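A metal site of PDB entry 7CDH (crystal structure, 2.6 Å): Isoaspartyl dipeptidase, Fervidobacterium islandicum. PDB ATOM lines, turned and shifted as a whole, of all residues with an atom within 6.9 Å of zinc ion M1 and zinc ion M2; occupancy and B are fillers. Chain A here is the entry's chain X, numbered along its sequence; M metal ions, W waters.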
ATOM      1  N   HIS A  61      -4.488 -12.525   1.702  1.00  0.00           N
ATOM      2  CA  HIS A  61      -4.581 -13.884   2.267  1.00  0.00           C
ATOM      3  C   HIS A  61      -3.843 -14.915   1.390  1.00  0.00           C
ATOM      4  O   HIS A  61      -4.468 -15.478   0.479  1.00  0.00           O
ATOM      5  CB  HIS A  61      -6.050 -14.218   2.476  1.00  0.00           C
ATOM      6  CG  HIS A  61      -6.245 -15.522   3.143  1.00  0.00           C
ATOM      7  ND1 HIS A  61      -6.447 -15.623   4.493  1.00  0.00           N
ATOM      8  CD2 HIS A  61      -6.202 -16.779   2.666  1.00  0.00           C
ATOM      9  CE1 HIS A  61      -6.569 -16.882   4.811  1.00  0.00           C
ATOM     10  NE2 HIS A  61      -6.386 -17.621   3.719  1.00  0.00           N
ATOM     11  N   VAL A  62      -2.541 -15.132   1.676  1.00  0.00           N
ATOM     12  CA  VAL A  62      -1.655 -16.108   0.964  1.00  0.00           C
ATOM     13  C   VAL A  62      -0.894 -16.991   1.954  1.00  0.00           C
ATOM     14  O   VAL A  62      -0.306 -16.493   2.897  1.00  0.00           O
ATOM     15  CB  VAL A  62      -0.675 -15.384   0.037  1.00  0.00           C
ATOM     16  CG1 VAL A  62       0.184 -16.350  -0.738  1.00  0.00           C
ATOM     17  CG2 VAL A  62      -1.437 -14.478  -0.915  1.00  0.00           C
ATOM     18  N   HIS A  63      -0.920 -18.298   1.738  1.00  0.00           N
ATOM     19  CA  HIS A  63      -0.114 -19.256   2.524  1.00  0.00           C
ATOM     20  C   HIS A  63       1.275 -19.257   1.930  1.00  0.00           C
ATOM     21  O   HIS A  63       1.566 -20.204   1.277  1.00  0.00           O
ATOM     22  CB  HIS A  63      -0.783 -20.620   2.560  1.00  0.00           C
ATOM     23  CG  HIS A  63      -2.092 -20.550   3.275  1.00  0.00           C
ATOM     24  ND1 HIS A  63      -2.162 -20.401   4.627  1.00  0.00           N
ATOM     25  CD2 HIS A  63      -3.365 -20.545   2.832  1.00  0.00           C
ATOM     26  CE1 HIS A  63      -3.435 -20.352   5.013  1.00  0.00           C
ATOM     27  NE2 HIS A  63      -4.199 -20.439   3.928  1.00  0.00           N
ATOM     28  N   CYS A  96      -0.246 -15.927   6.076  1.00  0.00           N
ATOM     29  CA  CYS A  96      -0.702 -16.562   7.324  1.00  0.00           C
ATOM     30  C   CYS A  96      -0.444 -18.067   7.283  1.00  0.00           C
ATOM     31  O   CYS A  96      -0.092 -18.600   6.198  1.00  0.00           O
ATOM     32  CB  CYS A  96      -2.185 -16.283   7.507  1.00  0.00           C
ATOM     33  SG  CYS A  96      -3.191 -16.886   6.129  1.00  0.00           S
ATOM     34  N   LEU A  97      -0.695 -18.717   8.422  1.00  0.00           N
ATOM     35  CA  LEU A  97      -0.805 -20.189   8.552  1.00  0.00           C
ATOM     36  C   LEU A  97      -2.272 -20.626   8.526  1.00  0.00           C
ATOM     37  O   LEU A  97      -3.159 -19.814   8.816  1.00  0.00           O
ATOM     38  CB  LEU A  97      -0.175 -20.660   9.873  1.00  0.00           C
ATOM     39  CG  LEU A  97       1.242 -20.186  10.125  1.00  0.00           C
ATOM     40  CD1 LEU A  97       1.736 -20.714  11.453  1.00  0.00           C
ATOM     41  CD2 LEU A  97       2.135 -20.651   8.992  1.00  0.00           C
ATOM     42  N   GLY A  98      -2.494 -21.906   8.268  1.00  0.00           N
ATOM     43  CA  GLY A  98      -3.834 -22.474   8.105  1.00  0.00           C
ATOM     44  C   GLY A  98      -4.080 -23.617   9.062  1.00  0.00           C
ATOM     45  O   GLY A  98      -3.750 -23.506  10.214  1.00  0.00           O
ATOM     46  N   TYR A 130      -5.224 -21.491  12.413  1.00  0.00           N
ATOM     47  CA  TYR A 130      -6.639 -21.902  12.589  1.00  0.00           C
ATOM     48  C   TYR A 130      -6.953 -22.056  14.066  1.00  0.00           C
ATOM     49  O   TYR A 130      -8.003 -21.623  14.502  1.00  0.00           O
ATOM     50  CB  TYR A 130      -6.937 -23.257  11.930  1.00  0.00           C
ATOM     51  CG  TYR A 130      -7.433 -23.246  10.512  1.00  0.00           C
ATOM     52  CD1 TYR A 130      -7.045 -22.297   9.573  1.00  0.00           C
ATOM     53  CD2 TYR A 130      -8.285 -24.255  10.087  1.00  0.00           C
ATOM     54  CE1 TYR A 130      -7.480 -22.336   8.260  1.00  0.00           C
ATOM     55  CE2 TYR A 130      -8.762 -24.300   8.783  1.00  0.00           C
ATOM     56  CZ  TYR A 130      -8.355 -23.351   7.865  1.00  0.00           C
ATOM     57  OH  TYR A 130      -8.819 -23.467   6.576  1.00  0.00           O
ATOM     58  N   GLU A 156      -5.230 -17.368  10.309  1.00  0.00           N
ATOM     59  CA  GLU A 156      -6.666 -17.233  10.131  1.00  0.00           C
ATOM     60  C   GLU A 156      -7.366 -18.139  11.152  1.00  0.00           C
ATOM     61  O   GLU A 156      -7.221 -19.354  11.069  1.00  0.00           O
ATOM     62  CB  GLU A 156      -7.092 -17.472   8.680  1.00  0.00           C
ATOM     63  CG  GLU A 156      -6.451 -18.662   8.038  1.00  0.00           C
ATOM     64  CD  GLU A 156      -7.029 -19.161   6.715  1.00  0.00           C
ATOM     65  OE1 GLU A 156      -8.262 -18.961   6.423  1.00  0.00           O
ATOM     66  OE2 GLU A 156      -6.213 -19.711   5.954  1.00  0.00           O
ATOM     67  N   ARG A 163     -12.545 -28.169  10.888  1.00  0.00           N
ATOM     68  CA  ARG A 163     -11.100 -28.104  11.246  1.00  0.00           C
ATOM     69  C   ARG A 163     -10.836 -27.074  12.362  1.00  0.00           C
ATOM     70  O   ARG A 163      -9.631 -26.864  12.750  1.00  0.00           O
ATOM     71  CB  ARG A 163     -10.251 -27.787  10.015  1.00  0.00           C
ATOM     72  CG  ARG A 163     -10.318 -28.844   8.920  1.00  0.00           C
ATOM     73  CD  ARG A 163      -9.957 -28.205   7.586  1.00  0.00           C
ATOM     74  NE  ARG A 163     -11.084 -27.402   7.094  1.00  0.00           N
ATOM     75  CZ  ARG A 163     -11.101 -26.717   5.950  1.00  0.00           C
ATOM     76  NH1 ARG A 163     -10.049 -26.676   5.157  1.00  0.00           N
ATOM     77  NH2 ARG A 163     -12.200 -26.058   5.618  1.00  0.00           N
ATOM     78  N   ASN A 193      -8.455 -12.118  11.253  1.00  0.00           N
ATOM     79  CA  ASN A 193      -8.922 -12.784  10.025  1.00  0.00           C
ATOM     80  C   ASN A 193      -9.587 -14.096  10.460  1.00  0.00           C
ATOM     81  O   ASN A 193      -8.913 -14.930  11.102  1.00  0.00           O
ATOM     82  CB  ASN A 193      -7.766 -12.934   9.037  1.00  0.00           C
ATOM     83  CG  ASN A 193      -8.134 -13.652   7.757  1.00  0.00           C
ATOM     84  OD1 ASN A 193      -7.381 -14.501   7.291  1.00  0.00           O
ATOM     85  ND2 ASN A 193      -9.222 -13.272   7.130  1.00  0.00           N
ATOM     86  N   PHE A 194     -10.881 -14.232  10.164  1.00  0.00           N
ATOM     87  CA  PHE A 194     -11.662 -15.450  10.487  1.00  0.00           C
ATOM     88  C   PHE A 194     -11.749 -16.284   9.217  1.00  0.00           C
ATOM     89  O   PHE A 194     -12.242 -15.768   8.211  1.00  0.00           O
ATOM     90  CB  PHE A 194     -13.064 -15.102  10.970  1.00  0.00           C
ATOM     91  CG  PHE A 194     -13.070 -14.388  12.283  1.00  0.00           C
ATOM     92  CD1 PHE A 194     -12.875 -15.077  13.465  1.00  0.00           C
ATOM     93  CD2 PHE A 194     -13.201 -13.014  12.347  1.00  0.00           C
ATOM     94  CE1 PHE A 194     -12.850 -14.411  14.681  1.00  0.00           C
ATOM     95  CE2 PHE A 194     -13.166 -12.349  13.564  1.00  0.00           C
ATOM     96  CZ  PHE A 194     -13.001 -13.057  14.726  1.00  0.00           C
ATOM     97  N   HIS A 195     -11.221 -17.517   9.274  1.00  0.00           N
ATOM     98  CA  HIS A 195     -11.617 -18.566   8.323  1.00  0.00           C
ATOM     99  C   HIS A 195     -13.049 -18.978   8.658  1.00  0.00           C
ATOM    100  O   HIS A 195     -13.278 -19.522   9.751  1.00  0.00           O
ATOM    101  CB  HIS A 195     -10.670 -19.749   8.367  1.00  0.00           C
ATOM    102  CG  HIS A 195     -11.203 -20.944   7.658  1.00  0.00           C
ATOM    103  ND1 HIS A 195     -10.828 -21.238   6.369  1.00  0.00           N
ATOM    104  CD2 HIS A 195     -12.121 -21.863   8.037  1.00  0.00           C
ATOM    105  CE1 HIS A 195     -11.479 -22.324   5.989  1.00  0.00           C
ATOM    106  NE2 HIS A 195     -12.286 -22.748   6.997  1.00  0.00           N
ATOM    107  N   VAL A 196     -13.985 -18.737   7.756  1.00  0.00           N
ATOM    108  CA  VAL A 196     -15.392 -19.146   8.002  1.00  0.00           C
ATOM    109  C   VAL A 196     -15.692 -20.389   7.176  1.00  0.00           C
ATOM    110  O   VAL A 196     -15.619 -20.320   5.943  1.00  0.00           O
ATOM    111  CB  VAL A 196     -16.403 -18.041   7.708  1.00  0.00           C
ATOM    112  CG1 VAL A 196     -17.794 -18.513   8.109  1.00  0.00           C
ATOM    113  CG2 VAL A 196     -16.041 -16.740   8.413  1.00  0.00           C
ATOM    114  N   THR A 223     -13.200 -14.270   5.941  1.00  0.00           N
ATOM    115  CA  THR A 223     -12.929 -14.663   4.533  1.00  0.00           C
ATOM    116  C   THR A 223     -13.823 -15.865   4.178  1.00  0.00           C
ATOM    117  O   THR A 223     -14.574 -16.312   5.050  1.00  0.00           O
ATOM    118  CB  THR A 223     -11.425 -14.857   4.287  1.00  0.00           C
ATOM    119  OG1 THR A 223     -11.240 -15.099   2.886  1.00  0.00           O
ATOM    120  CG2 THR A 223     -10.827 -15.996   5.094  1.00  0.00           C
ATOM    121  N   HIS A 224     -13.738 -16.342   2.926  1.00  0.00           N
ATOM    122  CA  HIS A 224     -14.599 -17.408   2.354  1.00  0.00           C
ATOM    123  C   HIS A 224     -16.061 -16.977   2.408  1.00  0.00           C
ATOM    124  O   HIS A 224     -16.918 -17.816   2.536  1.00  0.00           O
ATOM    125  CB  HIS A 224     -14.398 -18.757   3.074  1.00  0.00           C
ATOM    126  CG  HIS A 224     -12.952 -19.057   3.181  1.00  0.00           C
ATOM    127  ND1 HIS A 224     -12.114 -18.992   2.095  1.00  0.00           N
ATOM    128  CD2 HIS A 224     -12.180 -19.323   4.257  1.00  0.00           C
ATOM    129  CE1 HIS A 224     -10.886 -19.197   2.478  1.00  0.00           C
ATOM    130  NE2 HIS A 224     -10.896 -19.418   3.794  1.00  0.00           N
ATOM    131  N   ARG A 227     -18.649 -18.463  -0.008  1.00  0.00           N
ATOM    132  CA  ARG A 227     -18.757 -19.948   0.052  1.00  0.00           C
ATOM    133  C   ARG A 227     -20.194 -20.365  -0.295  1.00  0.00           C
ATOM    134  O   ARG A 227     -20.383 -21.388  -0.937  1.00  0.00           O
ATOM    135  CB  ARG A 227     -18.257 -20.374   1.435  1.00  0.00           C
ATOM    136  CG  ARG A 227     -18.539 -21.805   1.835  1.00  0.00           C
ATOM    137  CD  ARG A 227     -18.270 -22.063   3.317  1.00  0.00           C
ATOM    138  NE  ARG A 227     -16.907 -21.767   3.707  1.00  0.00           N
ATOM    139  CZ  ARG A 227     -15.851 -22.516   3.391  1.00  0.00           C
ATOM    140  NH1 ARG A 227     -14.634 -22.167   3.781  1.00  0.00           N
ATOM    141  NH2 ARG A 227     -16.011 -23.607   2.654  1.00  0.00           N
ATOM    142  N   THR A 248     -13.085 -15.498  -1.614  1.00  0.00           N
ATOM    143  CA  THR A 248     -11.963 -16.239  -2.228  1.00  0.00           C
ATOM    144  C   THR A 248     -12.095 -16.046  -3.740  1.00  0.00           C
ATOM    145  O   THR A 248     -13.135 -16.431  -4.310  1.00  0.00           O
ATOM    146  CB  THR A 248     -11.929 -17.697  -1.771  1.00  0.00           C
ATOM    147  OG1 THR A 248     -11.915 -17.692  -0.347  1.00  0.00           O
ATOM    148  CG2 THR A 248     -10.716 -18.403  -2.323  1.00  0.00           C
ATOM    149  N   ASP A 285      -6.049 -17.070  -1.592  1.00  0.00           N
ATOM    150  CA  ASP A 285      -5.770 -18.225  -0.699  1.00  0.00           C
ATOM    151  C   ASP A 285      -4.633 -19.040  -1.339  1.00  0.00           C
ATOM    152  O   ASP A 285      -4.740 -20.271  -1.423  1.00  0.00           O
ATOM    153  CB  ASP A 285      -7.032 -19.052  -0.502  1.00  0.00           C
ATOM    154  CG  ASP A 285      -7.010 -19.799   0.816  1.00  0.00           C
ATOM    155  OD1 ASP A 285      -6.091 -19.532   1.577  1.00  0.00           O
ATOM    156  OD2 ASP A 285      -7.951 -20.591   1.097  1.00  0.00           O
ATOM    157  N   GLY A 286      -3.636 -18.346  -1.872  1.00  0.00           N
ATOM    158  CA  GLY A 286      -2.592 -18.971  -2.697  1.00  0.00           C
ATOM    159  C   GLY A 286      -1.825 -20.005  -1.888  1.00  0.00           C
ATOM    160  O   GLY A 286      -1.590 -19.714  -0.720  1.00  0.00           O
ATOM    161  N   GLY A 288      -2.970 -22.555  -0.784  1.00  0.00           N
ATOM    162  CA  GLY A 288      -3.999 -23.221   0.017  1.00  0.00           C
ATOM    163  C   GLY A 288      -4.350 -24.568  -0.584  1.00  0.00           C
ATOM    164  O   GLY A 288      -3.919 -24.830  -1.741  1.00  0.00           O
HETATM  165 ZN    ZN M   1      -6.416 -19.719   3.919  1.00  0.00          ZN
HETATM  166 ZN    ZN M   2      -9.303 -20.462   5.125  1.00  0.00          ZN
HETATM  167  O   HOH W   1      -7.429 -22.450   4.699  1.00  0.00           O
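Tyr 130 touches zinc ion M2 (OH to ZN, 3.4 Å).
Of the 20 residues printed, 4 come within 4 Å of zinc ion M2.
The nearest printed residue that does not touch zinc ion M2 is Asp 285 (4.3 Å).
Of the 20 residues printed, 4 come within 4 Å of zinc ion M1.
Zinc ion M2 is bound by a ring nitrogen (ND1) of His 195, the side-chain carboxylate of Glu 156 and a ring nitrogen (NE2) of His 224.
Slightly farther from zinc ion M2 lies water W1 (2.8 Å).
The backbone carbonyl oxygen (O) of Glu 156 sits close to the backbone NH (N) of Tyr 130, at 3.2 Å.
A ring nitrogen (ND1) of His 61 lies within hydrogen-bond range of the side-chain amide oxygen (OD1) of Asn 193 (3.2 Å).
ND1 of His 195 sits close to OH of Tyr 130 (3.0 Å).
The side-chain hydroxyl (OG1) of Thr 248 sits at hydrogen-bond distance from a ring nitrogen (ND1) of His 224, 2.8 Å away.
ND1 of His 63 is in hydrogen-bond range of O of Cys 96, at 3.2 Å.
The backbone NH of His 63 sits at hydrogen-bond distance from the backbone carbonyl oxygen of Gly 286, 2.9 Å away.
O of Gly 98 lies within hydrogen-bond range of N of Tyr 130 (3.3 Å).
The side-chain carboxylate (OE2) of Glu 156 is bound to zinc ion M1, at 2.0 Å.
NE2 of His 61 is bound to zinc ion M1, at 2.1 Å.
Zinc ion M1 is bound by NE2 of His 63 (2.3 Å).
OD1 of Asp 285 is bound to zinc ion M1 (2.4 Å).
Zinc ion M1 has four donor atoms within binding distance.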
